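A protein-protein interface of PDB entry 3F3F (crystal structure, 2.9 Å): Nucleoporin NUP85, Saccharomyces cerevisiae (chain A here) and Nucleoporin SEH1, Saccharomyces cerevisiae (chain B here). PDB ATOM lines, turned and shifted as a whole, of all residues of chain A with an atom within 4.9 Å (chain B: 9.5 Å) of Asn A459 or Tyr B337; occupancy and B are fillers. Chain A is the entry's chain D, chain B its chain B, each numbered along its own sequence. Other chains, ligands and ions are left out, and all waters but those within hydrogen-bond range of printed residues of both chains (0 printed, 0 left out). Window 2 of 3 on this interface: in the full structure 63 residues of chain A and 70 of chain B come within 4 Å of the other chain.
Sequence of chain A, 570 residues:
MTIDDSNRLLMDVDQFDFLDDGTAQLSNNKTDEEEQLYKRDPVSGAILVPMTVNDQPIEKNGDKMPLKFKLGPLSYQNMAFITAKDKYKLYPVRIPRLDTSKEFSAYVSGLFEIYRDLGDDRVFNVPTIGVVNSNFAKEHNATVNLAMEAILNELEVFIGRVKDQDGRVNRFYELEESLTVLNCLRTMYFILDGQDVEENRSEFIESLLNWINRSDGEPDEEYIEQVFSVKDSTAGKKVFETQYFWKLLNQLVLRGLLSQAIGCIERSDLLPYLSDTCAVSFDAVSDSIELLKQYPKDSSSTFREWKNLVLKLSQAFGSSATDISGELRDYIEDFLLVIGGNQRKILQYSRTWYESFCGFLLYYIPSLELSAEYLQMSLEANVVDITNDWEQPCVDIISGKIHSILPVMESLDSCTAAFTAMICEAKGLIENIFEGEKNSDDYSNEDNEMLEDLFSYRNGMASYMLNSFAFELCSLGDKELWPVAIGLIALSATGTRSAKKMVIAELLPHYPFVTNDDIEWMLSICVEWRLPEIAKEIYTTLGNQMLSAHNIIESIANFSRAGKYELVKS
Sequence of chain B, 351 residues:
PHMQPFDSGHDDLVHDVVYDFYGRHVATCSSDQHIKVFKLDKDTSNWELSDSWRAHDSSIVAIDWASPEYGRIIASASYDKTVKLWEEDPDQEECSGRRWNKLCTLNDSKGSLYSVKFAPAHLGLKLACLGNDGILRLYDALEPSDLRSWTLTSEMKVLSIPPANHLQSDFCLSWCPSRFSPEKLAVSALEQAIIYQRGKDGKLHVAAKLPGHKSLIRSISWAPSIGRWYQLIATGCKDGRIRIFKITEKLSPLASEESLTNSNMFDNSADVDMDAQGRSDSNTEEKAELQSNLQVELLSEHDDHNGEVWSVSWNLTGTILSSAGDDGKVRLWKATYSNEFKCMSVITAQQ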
ATOM      1  N   ASN A 432       9.548 -25.399  31.589  1.00  0.00           N
ATOM      2  CA  ASN A 432       8.628 -24.350  32.002  1.00  0.00           C
ATOM      3  C   ASN A 432       9.104 -23.745  33.337  1.00  0.00           C
ATOM      4  O   ASN A 432       8.964 -24.357  34.401  1.00  0.00           O
ATOM      5  CB  ASN A 432       7.218 -24.952  32.121  1.00  0.00           C
ATOM      6  CG  ASN A 432       6.139 -23.908  32.396  1.00  0.00           C
ATOM      7  OD1 ASN A 432       6.144 -22.817  31.821  1.00  0.00           O
ATOM      8  ND2 ASN A 432       5.191 -24.255  33.265  1.00  0.00           N
ATOM      9  N   ASP A 453      -5.702 -19.996  30.026  1.00  0.00           N
ATOM     10  CA  ASP A 453      -5.095 -19.616  28.759  1.00  0.00           C
ATOM     11  C   ASP A 453      -4.231 -20.786  28.314  1.00  0.00           C
ATOM     12  O   ASP A 453      -3.025 -20.816  28.565  1.00  0.00           O
ATOM     13  CB  ASP A 453      -4.211 -18.357  28.911  1.00  0.00           C
ATOM     14  CG  ASP A 453      -4.992 -17.115  29.351  1.00  0.00           C
ATOM     15  OD1 ASP A 453      -6.217 -17.058  29.125  1.00  0.00           O
ATOM     16  OD2 ASP A 453      -4.372 -16.179  29.908  1.00  0.00           O
ATOM     17  N   LEU A 454      -4.863 -21.766  27.678  1.00  0.00           N
ATOM     18  CA  LEU A 454      -4.151 -22.934  27.192  1.00  0.00           C
ATOM     19  C   LEU A 454      -3.044 -22.381  26.316  1.00  0.00           C
ATOM     20  O   LEU A 454      -1.868 -22.449  26.679  1.00  0.00           O
ATOM     21  CB  LEU A 454      -5.095 -23.821  26.376  1.00  0.00           C
ATOM     22  CG  LEU A 454      -4.618 -25.228  26.011  1.00  0.00           C
ATOM     23  CD1 LEU A 454      -5.798 -26.083  25.617  1.00  0.00           C
ATOM     24  CD2 LEU A 454      -3.614 -25.163  24.890  1.00  0.00           C
ATOM     25  N   SER A 456      -0.987 -20.096  25.661  1.00  0.00           N
ATOM     26  CA  SER A 456      -0.241 -18.950  26.168  1.00  0.00           C
ATOM     27  C   SER A 456       1.159 -19.286  26.650  1.00  0.00           C
ATOM     28  O   SER A 456       1.628 -20.423  26.534  1.00  0.00           O
ATOM     29  CB  SER A 456      -0.999 -18.287  27.320  1.00  0.00           C
ATOM     30  OG  SER A 456      -0.995 -19.123  28.468  1.00  0.00           O
ATOM     31  N   TYR A 457       1.807 -18.267  27.209  1.00  0.00           N
ATOM     32  CA  TYR A 457       3.162 -18.375  27.740  1.00  0.00           C
ATOM     33  C   TYR A 457       3.119 -18.982  29.142  1.00  0.00           C
ATOM     34  O   TYR A 457       4.158 -19.259  29.747  1.00  0.00           O
ATOM     35  CB  TYR A 457       3.792 -16.986  27.811  1.00  0.00           C
ATOM     36  CG  TYR A 457       3.323 -16.177  28.996  1.00  0.00           C
ATOM     37  CD1 TYR A 457       3.899 -16.360  30.254  1.00  0.00           C
ATOM     38  CD2 TYR A 457       2.286 -15.253  28.871  1.00  0.00           C
ATOM     39  CE1 TYR A 457       3.462 -15.646  31.363  1.00  0.00           C
ATOM     40  CE2 TYR A 457       1.834 -14.527  29.978  1.00  0.00           C
ATOM     41  CZ  TYR A 457       2.430 -14.731  31.222  1.00  0.00           C
ATOM     42  OH  TYR A 457       2.008 -14.026  32.331  1.00  0.00           O
ATOM     43  N   ARG A 458       1.909 -19.166  29.659  1.00  0.00           N
ATOM     44  CA  ARG A 458       1.731 -19.728  30.992  1.00  0.00           C
ATOM     45  C   ARG A 458       2.345 -21.132  31.091  1.00  0.00           C
ATOM     46  O   ARG A 458       3.028 -21.458  32.069  1.00  0.00           O
ATOM     47  CB  ARG A 458       0.236 -19.774  31.353  1.00  0.00           C
ATOM     48  CG  ARG A 458      -0.460 -18.409  31.461  1.00  0.00           C
ATOM     49  CD  ARG A 458      -1.873 -18.562  32.045  1.00  0.00           C
ATOM     50  NE  ARG A 458      -1.927 -18.219  33.466  1.00  0.00           N
ATOM     51  CZ  ARG A 458      -2.594 -18.916  34.383  1.00  0.00           C
ATOM     52  NH1 ARG A 458      -3.271 -20.010  34.036  1.00  0.00           N
ATOM     53  NH2 ARG A 458      -2.582 -18.513  35.650  1.00  0.00           N
ATOM     54  N   ASN A 459       2.091 -21.958  30.079  1.00  0.00           N
ATOM     55  CA  ASN A 459       2.633 -23.308  30.060  1.00  0.00           C
ATOM     56  C   ASN A 459       3.997 -23.248  29.383  1.00  0.00           C
ATOM     57  O   ASN A 459       4.616 -22.186  29.339  1.00  0.00           O
ATOM     58  CB  ASN A 459       1.677 -24.240  29.319  1.00  0.00           C
ATOM     59  CG  ASN A 459       0.292 -24.251  29.941  1.00  0.00           C
ATOM     60  OD1 ASN A 459       0.139 -24.536  31.130  1.00  0.00           O
ATOM     61  ND2 ASN A 459      -0.723 -23.936  29.142  1.00  0.00           N
ATOM     62  N   GLY A 460       4.467 -24.365  28.844  1.00  0.00           N
ATOM     63  CA  GLY A 460       5.778 -24.357  28.217  1.00  0.00           C
ATOM     64  C   GLY A 460       5.953 -23.534  26.953  1.00  0.00           C
ATOM     65  O   GLY A 460       5.022 -22.896  26.470  1.00  0.00           O
ATOM     66  N   MET A 461       7.176 -23.524  26.442  1.00  0.00           N
ATOM     67  CA  MET A 461       7.468 -22.834  25.203  1.00  0.00           C
ATOM     68  C   MET A 461       7.173 -23.890  24.141  1.00  0.00           C
ATOM     69  O   MET A 461       6.872 -23.585  22.977  1.00  0.00           O
ATOM     70  CB  MET A 461       8.942 -22.432  25.140  1.00  0.00           C
ATOM     71  CG  MET A 461       9.395 -21.886  23.772  1.00  0.00           C
ATOM     72  SD  MET A 461       8.563 -20.362  23.227  1.00  0.00           S
ATOM     73  CE  MET A 461       8.890 -20.337  21.408  1.00  0.00           C
ATOM     74  N   SER A 463       4.856 -26.486  24.750  1.00  0.00           N
ATOM     75  CA  SER A 463       3.417 -26.638  24.772  1.00  0.00           C
ATOM     76  C   SER A 463       2.861 -25.593  23.805  1.00  0.00           C
ATOM     77  O   SER A 463       2.075 -25.912  22.913  1.00  0.00           O
ATOM     78  CB  SER A 463       2.898 -26.409  26.186  1.00  0.00           C
ATOM     79  OG  SER A 463       1.563 -26.860  26.304  1.00  0.00           O
ATOM     80  N   TYR A 464       3.318 -24.353  23.968  1.00  0.00           N
ATOM     81  CA  TYR A 464       2.897 -23.236  23.126  1.00  0.00           C
ATOM     82  C   TYR A 464       3.015 -23.553  21.636  1.00  0.00           C
ATOM     83  O   TYR A 464       2.044 -23.449  20.888  1.00  0.00           O
ATOM     84  CB  TYR A 464       3.741 -21.988  23.434  1.00  0.00           C
ATOM     85  CG  TYR A 464       3.295 -20.734  22.702  1.00  0.00           C
ATOM     86  CD1 TYR A 464       2.190 -19.996  23.141  1.00  0.00           C
ATOM     87  CD2 TYR A 464       3.969 -20.284  21.568  1.00  0.00           C
ATOM     88  CE1 TYR A 464       1.770 -18.842  22.471  1.00  0.00           C
ATOM     89  CE2 TYR A 464       3.557 -19.133  20.888  1.00  0.00           C
ATOM     90  CZ  TYR A 464       2.456 -18.417  21.348  1.00  0.00           C
ATOM     91  OH  TYR A 464       2.032 -17.282  20.697  1.00  0.00           O
ATOM     92  N   THR A 494       0.068 -30.162  29.248  1.00  0.00           N
ATOM     93  CA  THR A 494      -0.368 -29.124  30.175  1.00  0.00           C
ATOM     94  C   THR A 494      -1.729 -28.562  29.797  1.00  0.00           C
ATOM     95  O   THR A 494      -2.091 -28.530  28.620  1.00  0.00           O
ATOM     96  CB  THR A 494       0.642 -27.981  30.226  1.00  0.00           C
ATOM     97  OG1 THR A 494       1.032 -27.632  28.892  1.00  0.00           O
ATOM     98  CG2 THR A 494       1.865 -28.395  31.032  1.00  0.00           C
ATOM     99  N   GLY A 495      -2.474 -28.114  30.804  1.00  0.00           N
ATOM    100  CA  GLY A 495      -3.796 -27.577  30.554  1.00  0.00           C
ATOM    101  C   GLY A 495      -4.878 -28.508  31.074  1.00  0.00           C
ATOM    102  O   GLY A 495      -4.799 -29.734  30.925  1.00  0.00           O
ATOM    103  N   GLY B 227      -8.850 -21.032  23.047  1.00  0.00           N
ATOM    104  CA  GLY B 227      -7.697 -21.286  23.883  1.00  0.00           C
ATOM    105  C   GLY B 227      -7.407 -20.195  24.899  1.00  0.00           C
ATOM    106  O   GLY B 227      -7.117 -20.505  26.051  1.00  0.00           O
ATOM    107  N   TYR B 230      -8.672 -14.115  27.694  1.00  0.00           N
ATOM    108  CA  TYR B 230      -8.846 -12.709  27.383  1.00  0.00           C
ATOM    109  C   TYR B 230      -9.404 -12.561  25.963  1.00  0.00           C
ATOM    110  O   TYR B 230      -9.529 -13.541  25.215  1.00  0.00           O
ATOM    111  CB  TYR B 230      -7.511 -11.972  27.482  1.00  0.00           C
ATOM    112  CG  TYR B 230      -6.377 -12.577  26.668  1.00  0.00           C
ATOM    113  CD1 TYR B 230      -5.594 -13.612  27.182  1.00  0.00           C
ATOM    114  CD2 TYR B 230      -6.055 -12.081  25.396  1.00  0.00           C
ATOM    115  CE1 TYR B 230      -4.514 -14.133  26.457  1.00  0.00           C
ATOM    116  CE2 TYR B 230      -4.979 -12.595  24.663  1.00  0.00           C
ATOM    117  CZ  TYR B 230      -4.214 -13.615  25.201  1.00  0.00           C
ATOM    118  OH  TYR B 230      -3.136 -14.092  24.490  1.00  0.00           O
ATOM    119  N   LYS B 334       1.375 -12.223  13.587  1.00  0.00           N
ATOM    120  CA  LYS B 334       1.256 -13.331  14.531  1.00  0.00           C
ATOM    121  C   LYS B 334       1.661 -12.747  15.872  1.00  0.00           C
ATOM    122  O   LYS B 334       2.356 -11.744  15.921  1.00  0.00           O
ATOM    123  CB  LYS B 334       2.214 -14.477  14.167  1.00  0.00           C
ATOM    124  CG  LYS B 334       1.720 -15.434  13.077  1.00  0.00           C
ATOM    125  CD  LYS B 334       1.423 -16.843  13.637  1.00  0.00           C
ATOM    126  CE  LYS B 334       0.951 -17.825  12.529  1.00  0.00           C
ATOM    127  NZ  LYS B 334       0.515 -19.189  13.017  1.00  0.00           N
ATOM    128  N   ALA B 335       1.233 -13.357  16.962  1.00  0.00           N
ATOM    129  CA  ALA B 335       1.602 -12.836  18.265  1.00  0.00           C
ATOM    130  C   ALA B 335       2.884 -13.496  18.751  1.00  0.00           C
ATOM    131  O   ALA B 335       3.099 -14.689  18.516  1.00  0.00           O
ATOM    132  CB  ALA B 335       0.485 -13.080  19.254  1.00  0.00           C
ATOM    133  N   THR B 336       3.741 -12.719  19.413  1.00  0.00           N
ATOM    134  CA  THR B 336       4.995 -13.236  19.957  1.00  0.00           C
ATOM    135  C   THR B 336       4.660 -14.025  21.203  1.00  0.00           C
ATOM    136  O   THR B 336       3.505 -14.085  21.623  1.00  0.00           O
ATOM    137  CB  THR B 336       5.959 -12.127  20.406  1.00  0.00           C
ATOM    138  OG1 THR B 336       5.397 -10.849  20.119  1.00  0.00           O
ATOM    139  CG2 THR B 336       7.283 -12.261  19.696  1.00  0.00           C
ATOM    140  N   TYR B 337       5.681 -14.625  21.798  1.00  0.00           N
ATOM    141  CA  TYR B 337       5.500 -15.404  23.010  1.00  0.00           C
ATOM    142  C   TYR B 337       5.180 -14.416  24.139  1.00  0.00           C
ATOM    143  O   TYR B 337       4.543 -14.768  25.135  1.00  0.00           O
ATOM    144  CB  TYR B 337       6.794 -16.177  23.298  1.00  0.00           C
ATOM    145  CG  TYR B 337       6.695 -17.201  24.406  1.00  0.00           C
ATOM    146  CD1 TYR B 337       5.851 -18.296  24.294  1.00  0.00           C
ATOM    147  CD2 TYR B 337       7.459 -17.076  25.563  1.00  0.00           C
ATOM    148  CE1 TYR B 337       5.774 -19.244  25.308  1.00  0.00           C
ATOM    149  CE2 TYR B 337       7.386 -18.018  26.578  1.00  0.00           C
ATOM    150  CZ  TYR B 337       6.545 -19.099  26.444  1.00  0.00           C
ATOM    151  OH  TYR B 337       6.502 -20.045  27.441  1.00  0.00           O
ATOM    152  N   SER B 338       5.620 -13.171  23.949  1.00  0.00           N
ATOM    153  CA  SER B 338       5.418 -12.100  24.923  1.00  0.00           C
ATOM    154  C   SER B 338       4.082 -11.401  24.711  1.00  0.00           C
ATOM    155  O   SER B 338       3.719 -10.509  25.485  1.00  0.00           O
ATOM    156  CB  SER B 338       6.542 -11.068  24.822  1.00  0.00           C
ATOM    157  OG  SER B 338       6.625 -10.547  23.503  1.00  0.00           O
ATOM    158  N   ASN B 339       3.372 -11.796  23.656  1.00  0.00           N
ATOM    159  CA  ASN B 339       2.056 -11.245  23.336  1.00  0.00           C
ATOM    160  C   ASN B 339       2.109  -9.928  22.575  1.00  0.00           C
ATOM    161  O   ASN B 339       1.113  -9.207  22.496  1.00  0.00           O
ATOM    162  CB  ASN B 339       1.209 -11.074  24.606  1.00  0.00           C
ATOM    163  CG  ASN B 339      -0.248 -11.468  24.396  1.00  0.00           C
ATOM    164  OD1 ASN B 339      -0.650 -11.857  23.287  1.00  0.00           O
ATOM    165  ND2 ASN B 339      -1.050 -11.372  25.467  1.00  0.00           N
ATOM    166  N   GLU B 340       3.279  -9.602  22.045  1.00  0.00           N
ATOM    167  CA  GLU B 340       3.428  -8.410  21.220  1.00  0.00           C
ATOM    168  C   GLU B 340       2.995  -8.963  19.840  1.00  0.00           C
ATOM    169  O   GLU B 340       2.698 -10.155  19.732  1.00  0.00           O
ATOM    170  CB  GLU B 340       4.901  -7.975  21.234  1.00  0.00           C
ATOM    171  CG  GLU B 340       5.331  -6.972  20.158  1.00  0.00           C
ATOM    172  CD  GLU B 340       4.564  -5.658  20.189  1.00  0.00           C
ATOM    173  OE1 GLU B 340       4.668  -4.906  21.193  1.00  0.00           O
ATOM    174  OE2 GLU B 340       3.860  -5.383  19.190  1.00  0.00           O
ATOM    175  N   PHE B 341       2.908  -8.142  18.797  1.00  0.00           N
ATOM    176  CA  PHE B 341       2.535  -8.697  17.497  1.00  0.00           C
ATOM    177  C   PHE B 341       3.603  -8.379  16.492  1.00  0.00           C
ATOM    178  O   PHE B 341       4.120  -7.274  16.456  1.00  0.00           O
ATOM    179  CB  PHE B 341       1.185  -8.181  17.021  1.00  0.00           C
ATOM    180  CG  PHE B 341       0.037  -9.024  17.474  1.00  0.00           C
ATOM    181  CD1 PHE B 341      -0.390  -8.990  18.796  1.00  0.00           C
ATOM    182  CD2 PHE B 341      -0.598  -9.887  16.585  1.00  0.00           C
ATOM    183  CE1 PHE B 341      -1.438  -9.809  19.235  1.00  0.00           C
ATOM    184  CE2 PHE B 341      -1.643 -10.712  17.006  1.00  0.00           C
ATOM    185  CZ  PHE B 341      -2.065 -10.672  18.338  1.00  0.00           C
ATOM    186  N   LYS B 342       3.928  -9.358  15.667  1.00  0.00           N
ATOM    187  CA  LYS B 342       4.996  -9.207  14.697  1.00  0.00           C
ATOM    188  C   LYS B 342       4.507  -9.487  13.290  1.00  0.00           C
ATOM    189  O   LYS B 342       3.718 -10.405  13.067  1.00  0.00           O
ATOM    190  CB  LYS B 342       6.120 -10.182  15.069  1.00  0.00           C
ATOM    191  CG  LYS B 342       7.514  -9.784  14.640  1.00  0.00           C
ATOM    192  CD  LYS B 342       8.519 -10.826  15.103  1.00  0.00           C
ATOM    193  CE  LYS B 342       9.951 -10.391  14.803  1.00  0.00           C
ATOM    194  NZ  LYS B 342      10.945 -11.429  15.204  1.00  0.00           N
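N of Leu A454 lies within hydrogen-bond range of O of Gly B227 (3.1 Å).
OH of Tyr B337 is in hydrogen-bond range of O of Tyr A457, 3.4 Å away.
O of Asn A459 is in hydrogen-bond range of OH of Tyr B337 (3.4 Å).
The side-chain hydroxyl of Tyr B337 sits at hydrogen-bond distance from the backbone carbonyl oxygen of Gly A460 (3.4 Å).
The side-chain hydroxyl (OG1) of Thr B336 sits at hydrogen-bond distance from the backbone carbonyl oxygen (O) of Glu B340 (2.8 Å).
The backbone carbonyl oxygen (O) of Asn A459 sits close to the side-chain amide oxygen (OD1) of Asn A432, at 3.0 Å.
The side-chain hydroxyl of Ser A456 is in hydrogen-bond range of the backbone carbonyl oxygen of Asp A453 (2.6 Å).
The backbone carbonyl oxygen of Leu A454 lies within hydrogen-bond range of the side-chain amide nitrogen of Asn A459 (3.1 Å).
O of Gly B227 touches CA of Asp A453, 3.5 Å away.
Tyr B230 touches Asp A453.
Met A461 touches Tyr B337.
Ala B335 touches Tyr A464 (O to OH, 3.6 Å).
Tyr A464 touches Thr B336.
Tyr B337 touches Tyr A464 (CD1 to CD2, 3.9 Å).
Of the printed residues of chain B, Asp A453 touches Gly B227 (3.5 Å) and Tyr B230 (3.9 Å).
Printed residues of chain B within 4 Å of Tyr A457: Tyr B337.
Asn A459 touches just one residue of chain B: Tyr B337.
Of chain B, only Tyr B337 comes within 4 Å of Met A461.
Ser A463 touches none of the printed residues of chain B.
Of the printed residues of chain B, Tyr A464 touches Ala B335, Thr B336 and Tyr B337.
Printed residues of chain A within 4 Å of Thr B336: Tyr A464 (3.6 Å).
Tyr B337 touches five residues of chain A.
Lys B342 touches none of the printed residues of chain A.
The nearest residue of chain B that does not touch Asn A459 is Gly B227 (7.9 Å).
The nearest printed residue of chain B that does not touch Leu A454 is Tyr B230 (7.7 Å).
Of the 11 printed residues of chain B, 5 touch a printed residue of chain A.
Printed residues of chain A that touch a printed residue of chain B: Asp A453, Leu A454, Tyr A457, Asn A459, Gly A460, Met A461 and Tyr A464.
Among the printed residues, no Asp or Glu carboxylate lies within 4 Å of a Lys or Arg side-chain nitrogen of the other chain.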
